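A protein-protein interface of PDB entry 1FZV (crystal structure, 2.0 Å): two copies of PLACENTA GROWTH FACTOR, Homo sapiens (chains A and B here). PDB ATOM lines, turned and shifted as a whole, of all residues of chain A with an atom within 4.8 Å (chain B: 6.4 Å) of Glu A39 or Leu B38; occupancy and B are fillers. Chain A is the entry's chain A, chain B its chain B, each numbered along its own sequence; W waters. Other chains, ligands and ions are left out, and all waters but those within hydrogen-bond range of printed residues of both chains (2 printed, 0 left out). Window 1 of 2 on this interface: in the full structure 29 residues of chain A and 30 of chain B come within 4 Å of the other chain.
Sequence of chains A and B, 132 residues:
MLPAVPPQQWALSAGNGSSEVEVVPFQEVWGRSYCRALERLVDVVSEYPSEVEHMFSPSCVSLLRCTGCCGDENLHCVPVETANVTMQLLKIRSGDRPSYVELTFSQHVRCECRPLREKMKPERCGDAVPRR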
ATOM      1  N   ALA A  37       6.273  -9.496  -6.584  1.00  0.00           N
ATOM      2  CA  ALA A  37       6.865  -8.869  -7.770  1.00  0.00           C
ATOM      3  C   ALA A  37       8.263  -9.459  -7.801  1.00  0.00           C
ATOM      4  O   ALA A  37       9.084  -9.124  -6.964  1.00  0.00           O
ATOM      5  CB  ALA A  37       6.948  -7.366  -7.585  1.00  0.00           C
ATOM      6  N   LEU A  38       8.511 -10.360  -8.736  1.00  0.00           N
ATOM      7  CA  LEU A  38       9.824 -11.013  -8.831  1.00  0.00           C
ATOM      8  C   LEU A  38      10.563 -10.716 -10.144  1.00  0.00           C
ATOM      9  O   LEU A  38       9.979 -10.808 -11.237  1.00  0.00           O
ATOM     10  CB  LEU A  38       9.631 -12.523  -8.709  1.00  0.00           C
ATOM     11  CG  LEU A  38      10.799 -13.454  -8.406  1.00  0.00           C
ATOM     12  CD1 LEU A  38      11.152 -13.361  -6.955  1.00  0.00           C
ATOM     13  CD2 LEU A  38      10.404 -14.869  -8.721  1.00  0.00           C
ATOM     14  N   GLU A  39      11.845 -10.382 -10.034  1.00  0.00           N
ATOM     15  CA  GLU A  39      12.662 -10.127 -11.216  1.00  0.00           C
ATOM     16  C   GLU A  39      12.673 -11.385 -12.056  1.00  0.00           C
ATOM     17  O   GLU A  39      12.953 -12.480 -11.567  1.00  0.00           O
ATOM     18  CB  GLU A  39      14.107  -9.752 -10.828  1.00  0.00           C
ATOM     19  CG  GLU A  39      15.038  -9.601 -12.041  1.00  0.00           C
ATOM     20  CD  GLU A  39      16.470  -9.223 -11.673  1.00  0.00           C
ATOM     21  OE1 GLU A  39      17.176  -8.715 -12.560  1.00  0.00           O
ATOM     22  OE2 GLU A  39      16.900  -9.427 -10.518  1.00  0.00           O
ATOM     23  N   ARG A  40      12.353 -11.220 -13.326  1.00  0.00           N
ATOM     24  CA  ARG A  40      12.313 -12.317 -14.281  1.00  0.00           C
ATOM     25  C   ARG A  40      12.960 -11.836 -15.579  1.00  0.00           C
ATOM     26  O   ARG A  40      12.876 -10.654 -15.911  1.00  0.00           O
ATOM     27  CB  ARG A  40      10.862 -12.688 -14.571  1.00  0.00           C
ATOM     28  CG  ARG A  40      10.697 -13.809 -15.560  1.00  0.00           C
ATOM     29  CD  ARG A  40       9.246 -13.938 -15.992  1.00  0.00           C
ATOM     30  NE  ARG A  40       9.036 -15.061 -16.902  1.00  0.00           N
ATOM     31  CZ  ARG A  40       9.121 -16.343 -16.544  1.00  0.00           C
ATOM     32  NH1 ARG A  40       9.411 -16.673 -15.287  1.00  0.00           N
ATOM     33  NH2 ARG A  40       8.917 -17.301 -17.444  1.00  0.00           N
ATOM     34  N   LEU A  41      13.580 -12.744 -16.322  1.00  0.00           N
ATOM     35  CA  LEU A  41      14.198 -12.354 -17.595  1.00  0.00           C
ATOM     36  C   LEU A  41      13.215 -12.739 -18.683  1.00  0.00           C
ATOM     37  O   LEU A  41      12.869 -13.908 -18.837  1.00  0.00           O
ATOM     38  CB  LEU A  41      15.540 -13.072 -17.790  1.00  0.00           C
ATOM     39  CG  LEU A  41      16.559 -12.900 -16.655  1.00  0.00           C
ATOM     40  CD1 LEU A  41      17.913 -13.479 -17.102  1.00  0.00           C
ATOM     41  CD2 LEU A  41      16.715 -11.440 -16.296  1.00  0.00           C
ATOM     42  N   SER A  62      15.403  -7.832 -18.048  1.00  0.00           N
ATOM     43  CA  SER A  62      15.008  -8.097 -16.669  1.00  0.00           C
ATOM     44  C   SER A  62      13.863  -7.154 -16.251  1.00  0.00           C
ATOM     45  O   SER A  62      14.045  -5.937 -16.178  1.00  0.00           O
ATOM     46  CB  SER A  62      16.219  -7.901 -15.764  1.00  0.00           C
ATOM     47  OG  SER A  62      15.890  -7.821 -14.387  1.00  0.00           O
ATOM     48  N   LEU A  63      12.690  -7.737 -15.994  1.00  0.00           N
ATOM     49  CA  LEU A  63      11.488  -6.996 -15.578  1.00  0.00           C
ATOM     50  C   LEU A  63      10.905  -7.612 -14.291  1.00  0.00           C
ATOM     51  O   LEU A  63      11.133  -8.796 -13.994  1.00  0.00           O
ATOM     52  CB  LEU A  63      10.426  -7.060 -16.695  1.00  0.00           C
ATOM     53  CG  LEU A  63      10.850  -6.453 -18.048  1.00  0.00           C
ATOM     54  CD1 LEU A  63       9.864  -6.784 -19.150  1.00  0.00           C
ATOM     55  CD2 LEU A  63      10.996  -4.972 -17.893  1.00  0.00           C
ATOM     56  N   LEU A  64      10.177  -6.808 -13.521  1.00  0.00           N
ATOM     57  CA  LEU A  64       9.547  -7.325 -12.305  1.00  0.00           C
ATOM     58  C   LEU A  64       8.190  -7.805 -12.789  1.00  0.00           C
ATOM     59  O   LEU A  64       7.453  -7.055 -13.419  1.00  0.00           O
ATOM     60  CB  LEU A  64       9.364  -6.237 -11.245  1.00  0.00           C
ATOM     61  CG  LEU A  64      10.614  -5.573 -10.651  1.00  0.00           C
ATOM     62  CD1 LEU A  64      10.172  -4.480  -9.699  1.00  0.00           C
ATOM     63  CD2 LEU A  64      11.495  -6.594  -9.915  1.00  0.00           C
ATOM     64  N   ARG B  32      22.322  -6.959 -16.803  1.00  0.00           N
ATOM     65  CA  ARG B  32      21.222  -7.383 -15.956  1.00  0.00           C
ATOM     66  C   ARG B  32      20.581  -8.675 -16.468  1.00  0.00           C
ATOM     67  O   ARG B  32      20.160  -9.518 -15.681  1.00  0.00           O
ATOM     68  CB  ARG B  32      20.166  -6.274 -15.891  1.00  0.00           C
ATOM     69  CG  ARG B  32      19.193  -6.424 -14.742  1.00  0.00           C
ATOM     70  CD  ARG B  32      19.782  -5.890 -13.450  1.00  0.00           C
ATOM     71  NE  ARG B  32      18.999  -6.318 -12.298  1.00  0.00           N
ATOM     72  CZ  ARG B  32      19.207  -5.898 -11.058  1.00  0.00           C
ATOM     73  NH1 ARG B  32      20.177  -5.034 -10.810  1.00  0.00           N
ATOM     74  NH2 ARG B  32      18.443  -6.341 -10.066  1.00  0.00           N
ATOM     75  N   SER B  33      20.507  -8.842 -17.786  1.00  0.00           N
ATOM     76  CA  SER B  33      19.896 -10.034 -18.344  1.00  0.00           C
ATOM     77  C   SER B  33      20.877 -11.089 -18.816  1.00  0.00           C
ATOM     78  O   SER B  33      20.484 -12.106 -19.378  1.00  0.00           O
ATOM     79  CB  SER B  33      18.957  -9.663 -19.491  1.00  0.00           C
ATOM     80  OG  SER B  33      19.627  -8.985 -20.518  1.00  0.00           O
ATOM     81  N   ARG B  36      22.890 -15.755 -15.531  1.00  0.00           N
ATOM     82  CA  ARG B  36      23.098 -15.674 -14.094  1.00  0.00           C
ATOM     83  C   ARG B  36      22.187 -16.642 -13.327  1.00  0.00           C
ATOM     84  O   ARG B  36      21.202 -17.126 -13.863  1.00  0.00           O
ATOM     85  CB  ARG B  36      22.814 -14.235 -13.639  1.00  0.00           C
ATOM     86  CG  ARG B  36      21.423 -13.734 -14.095  1.00  0.00           C
ATOM     87  CD  ARG B  36      21.261 -12.218 -13.921  1.00  0.00           C
ATOM     88  NE  ARG B  36      21.010 -11.856 -12.531  1.00  0.00           N
ATOM     89  CZ  ARG B  36      20.079 -10.981 -12.155  1.00  0.00           C
ATOM     90  NH1 ARG B  36      19.329 -10.379 -13.072  1.00  0.00           N
ATOM     91  NH2 ARG B  36      19.872 -10.732 -10.867  1.00  0.00           N
ATOM     92  N   ALA B  37      22.552 -16.927 -12.083  1.00  0.00           N
ATOM     93  CA  ALA B  37      21.769 -17.798 -11.201  1.00  0.00           C
ATOM     94  C   ALA B  37      20.688 -16.864 -10.659  1.00  0.00           C
ATOM     95  O   ALA B  37      20.981 -15.973  -9.860  1.00  0.00           O
ATOM     96  CB  ALA B  37      22.641 -18.303 -10.059  1.00  0.00           C
ATOM     97  N   LEU B  38      19.451 -17.055 -11.091  1.00  0.00           N
ATOM     98  CA  LEU B  38      18.376 -16.168 -10.658  1.00  0.00           C
ATOM     99  C   LEU B  38      17.241 -16.859  -9.890  1.00  0.00           C
ATOM    100  O   LEU B  38      16.733 -17.902 -10.312  1.00  0.00           O
ATOM    101  CB  LEU B  38      17.801 -15.460 -11.885  1.00  0.00           C
ATOM    102  CG  LEU B  38      16.824 -14.291 -11.746  1.00  0.00           C
ATOM    103  CD1 LEU B  38      17.552 -13.057 -11.254  1.00  0.00           C
ATOM    104  CD2 LEU B  38      16.205 -14.007 -13.091  1.00  0.00           C
ATOM    105  N   GLU B  39      16.852 -16.273  -8.762  1.00  0.00           N
ATOM    106  CA  GLU B  39      15.747 -16.826  -7.979  1.00  0.00           C
ATOM    107  C   GLU B  39      14.541 -16.930  -8.892  1.00  0.00           C
ATOM    108  O   GLU B  39      14.163 -15.967  -9.562  1.00  0.00           O
ATOM    109  CB  GLU B  39      15.402 -15.924  -6.786  1.00  0.00           C
ATOM    110  CG  GLU B  39      14.162 -16.384  -6.012  1.00  0.00           C
ATOM    111  CD  GLU B  39      13.936 -15.585  -4.738  1.00  0.00           C
ATOM    112  OE1 GLU B  39      13.237 -16.096  -3.837  1.00  0.00           O
ATOM    113  OE2 GLU B  39      14.451 -14.453  -4.628  1.00  0.00           O
ATOM    114  N   ARG B  40      13.949 -18.114  -8.922  1.00  0.00           N
ATOM    115  CA  ARG B  40      12.784 -18.397  -9.743  1.00  0.00           C
ATOM    116  C   ARG B  40      11.818 -19.227  -8.905  1.00  0.00           C
ATOM    117  O   ARG B  40      12.259 -20.016  -8.081  1.00  0.00           O
ATOM    118  CB  ARG B  40      13.208 -19.214 -10.955  1.00  0.00           C
ATOM    119  CG  ARG B  40      12.127 -19.399 -11.983  1.00  0.00           C
ATOM    120  CD  ARG B  40      12.285 -20.746 -12.673  1.00  0.00           C
ATOM    121  NE  ARG B  40      11.811 -20.715 -14.053  1.00  0.00           N
ATOM    122  CZ  ARG B  40      12.309 -19.910 -14.989  1.00  0.00           C
ATOM    123  NH1 ARG B  40      13.298 -19.072 -14.682  1.00  0.00           N
ATOM    124  NH2 ARG B  40      11.817 -19.932 -16.225  1.00  0.00           N
ATOM    125  N   LEU B  63      13.717 -21.372  -6.083  1.00  0.00           N
ATOM    126  CA  LEU B  63      15.035 -21.986  -6.307  1.00  0.00           C
ATOM    127  C   LEU B  63      15.923 -21.102  -7.201  1.00  0.00           C
ATOM    128  O   LEU B  63      15.419 -20.277  -7.980  1.00  0.00           O
ATOM    129  CB  LEU B  63      14.881 -23.366  -6.984  1.00  0.00           C
ATOM    130  CG  LEU B  63      14.088 -24.491  -6.307  1.00  0.00           C
ATOM    131  CD1 LEU B  63      13.985 -25.699  -7.225  1.00  0.00           C
ATOM    132  CD2 LEU B  63      14.743 -24.869  -5.023  1.00  0.00           C
ATOM    133  N   LEU B  64      17.238 -21.262  -7.079  1.00  0.00           N
ATOM    134  CA  LEU B  64      18.147 -20.498  -7.948  1.00  0.00           C
ATOM    135  C   LEU B  64      18.250 -21.340  -9.208  1.00  0.00           C
ATOM    136  O   LEU B  64      18.534 -22.532  -9.145  1.00  0.00           O
ATOM    137  CB  LEU B  64      19.536 -20.317  -7.326  1.00  0.00           C
ATOM    138  CG  LEU B  64      19.616 -19.371  -6.126  1.00  0.00           C
ATOM    139  CD1 LEU B  64      21.032 -19.350  -5.602  1.00  0.00           C
ATOM    140  CD2 LEU B  64      19.169 -17.953  -6.499  1.00  0.00           C
ATOM    141  N   ARG B  65      17.940 -20.725 -10.339  1.00  0.00           N
ATOM    142  CA  ARG B  65      18.031 -21.395 -11.633  1.00  0.00           C
ATOM    143  C   ARG B  65      18.815 -20.511 -12.618  1.00  0.00           C
ATOM    144  O   ARG B  65      18.610 -19.289 -12.678  1.00  0.00           O
ATOM    145  CB  ARG B  65      16.633 -21.679 -12.202  1.00  0.00           C
ATOM    146  CG  ARG B  65      15.918 -22.860 -11.568  1.00  0.00           C
ATOM    147  CD  ARG B  65      16.520 -24.172 -12.027  1.00  0.00           C
ATOM    148  NE  ARG B  65      16.052 -25.344 -11.288  1.00  0.00           N
ATOM    149  CZ  ARG B  65      16.494 -25.716 -10.092  1.00  0.00           C
ATOM    150  NH1 ARG B  65      17.420 -25.016  -9.462  1.00  0.00           N
ATOM    151  NH2 ARG B  65      16.024 -26.819  -9.533  1.00  0.00           N
ATOM    152  N   CYS B  66      19.732 -21.121 -13.374  1.00  0.00           N
ATOM    153  CA  CYS B  66      20.496 -20.367 -14.372  1.00  0.00           C
ATOM    154  C   CYS B  66      19.535 -19.826 -15.400  1.00  0.00           C
ATOM    155  O   CYS B  66      18.754 -20.569 -15.992  1.00  0.00           O
ATOM    156  CB  CYS B  66      21.515 -21.257 -15.090  1.00  0.00           C
ATOM    157  SG  CYS B  66      22.894 -21.722 -14.030  1.00  0.00           S
ATOM    158  N   THR B  67      19.595 -18.531 -15.633  1.00  0.00           N
ATOM    159  CA  THR B  67      18.688 -17.930 -16.587  1.00  0.00           C
ATOM    160  C   THR B  67      19.403 -16.752 -17.209  1.00  0.00           C
ATOM    161  O   THR B  67      20.170 -16.056 -16.544  1.00  0.00           O
ATOM    162  CB  THR B  67      17.391 -17.393 -15.880  1.00  0.00           C
ATOM    163  OG1 THR B  67      16.873 -18.400 -15.007  1.00  0.00           O
ATOM    164  CG2 THR B  67      16.324 -17.050 -16.903  1.00  0.00           C
ATOM    165  N   HIS B 108      21.095 -23.988  -8.346  1.00  0.00           N
ATOM    166  CA  HIS B 108      22.095 -23.566  -9.321  1.00  0.00           C
ATOM    167  C   HIS B 108      22.878 -22.419  -8.690  1.00  0.00           C
ATOM    168  O   HIS B 108      22.339 -21.331  -8.500  1.00  0.00           O
ATOM    169  CB  HIS B 108      21.429 -23.093 -10.608  1.00  0.00           C
ATOM    170  CG  HIS B 108      20.835 -24.197 -11.427  1.00  0.00           C
ATOM    171  ND1 HIS B 108      20.281 -23.985 -12.668  1.00  0.00           N
ATOM    172  CD2 HIS B 108      20.743 -25.529 -11.200  1.00  0.00           C
ATOM    173  CE1 HIS B 108      19.881 -25.136 -13.176  1.00  0.00           C
ATOM    174  NE2 HIS B 108      20.151 -26.089 -12.302  1.00  0.00           N
ATOM    175  N   CYS B 111      26.520 -19.759 -13.002  1.00  0.00           N
ATOM    176  CA  CYS B 111      26.101 -20.049 -14.352  1.00  0.00           C
ATOM    177  C   CYS B 111      27.032 -19.461 -15.401  1.00  0.00           C
ATOM    178  O   CYS B 111      27.712 -18.485 -15.142  1.00  0.00           O
ATOM    179  CB  CYS B 111      24.709 -19.459 -14.568  1.00  0.00           C
ATOM    180  SG  CYS B 111      23.530 -19.976 -13.276  1.00  0.00           S
HETATM  181  O   HOH W   1      12.706 -15.190 -11.925  1.00  0.00           O
HETATM  182  O   HOH W   2      14.407 -13.184  -9.365  1.00  0.00           O
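The side-chain carboxylate (OE1) of Glu A39 is in salt-bridge range of the guanidinium group (NE) of Arg B32.
OE1 of Glu A39 is in salt-bridge range of NH1 of Arg B36 (2.8 Å).
The side-chain carboxylate (OE1) of Glu A39 is in hydrogen-bond range of the side-chain hydroxyl (OG) of Ser A62 (2.4 Å).
The guanidinium group (NH1) of Arg B36 lies within hydrogen-bond range of the backbone carbonyl oxygen (O) of Arg B32 (2.9 Å).
The backbone carbonyl oxygen of Arg B36 lies within hydrogen-bond range of the backbone NH of Thr B67 (2.8 Å).
The backbone NH (N) of Leu B38 is in hydrogen-bond range of the backbone carbonyl oxygen (O) of Arg B65 (2.9 Å).
The backbone carbonyl oxygen (O) of Arg B65 sits at hydrogen-bond distance from the side-chain hydroxyl (OG1) of Thr B67 (3.0 Å).
SG of Cys B111 is disulfide-bonded to SG of Cys B66.
Among the printed residues, merely in contact across the chains: Leu A41 with Thr B67 (3.5 Å), Ser A62 with Arg B32 (3.5 Å), Leu A41 with Ser B33 (3.7 Å), Leu A41 with Leu B38 (3.7 Å), Glu A39 with Leu B38 (3.8 Å) and Leu A41 with Arg B32 (3.99 Å).
Glu A39 touches three residues of chain B.
Leu B38 touches just these residues of chain A: Glu A39 and Leu A41.
Printed residues of chain B within 4 Å of Ser A62: Arg B32.
Of the printed residues of chain A, Thr B67 touches Leu A41 (3.5 Å).
Of the printed residues of chain A, Arg B32 touches Glu A39 (3.0 Å), Leu A41 (3.99 Å) and Ser A62 (3.5 Å).
Of the printed residues of chain A, Ser B33 touches Leu A41.
Arg A40 touches none of the printed residues of chain B.
His B108 touches none of the printed residues of chain A.
The nearest residue of chain B that does not touch Glu A39 is Glu B39 (4.2 Å).
The nearest residue of chain A that does not touch Leu B38 is Arg A40 (4.4 Å).
The nearest printed residue of chain A that does not touch Ser B33 is Ser A62 (4.3 Å).
Hydrophobic or aromatic side chains of chain A that line the printed part of chain B: Leu A41.
Printed residues of chain B that touch a printed residue of chain A: Arg B32, Ser B33, Arg B36, Leu B38 and Thr B67.
Among the printed residues, 8 pairs touch across the chains.
Among the printed residues, Asp or Glu carboxylates within 4 Å of a Lys or Arg side-chain nitrogen of the other chain: Glu A39 with Arg B32 and Glu A39 with Arg B36.
Glu A39 touches Leu B38, but with the chains exchanged Leu A38 does not touch Glu B39 (4.01 Å).
Water W2 lies within hydrogen-bond range of the backbone carbonyl oxygen (O) of Glu A39 (2.7 Å) and the backbone carbonyl oxygen (O) of Glu B39 (2.8 Å).
Water W1 bridges O of Glu A39 (2.7 Å) and O of Glu B39 (2.9 Å).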
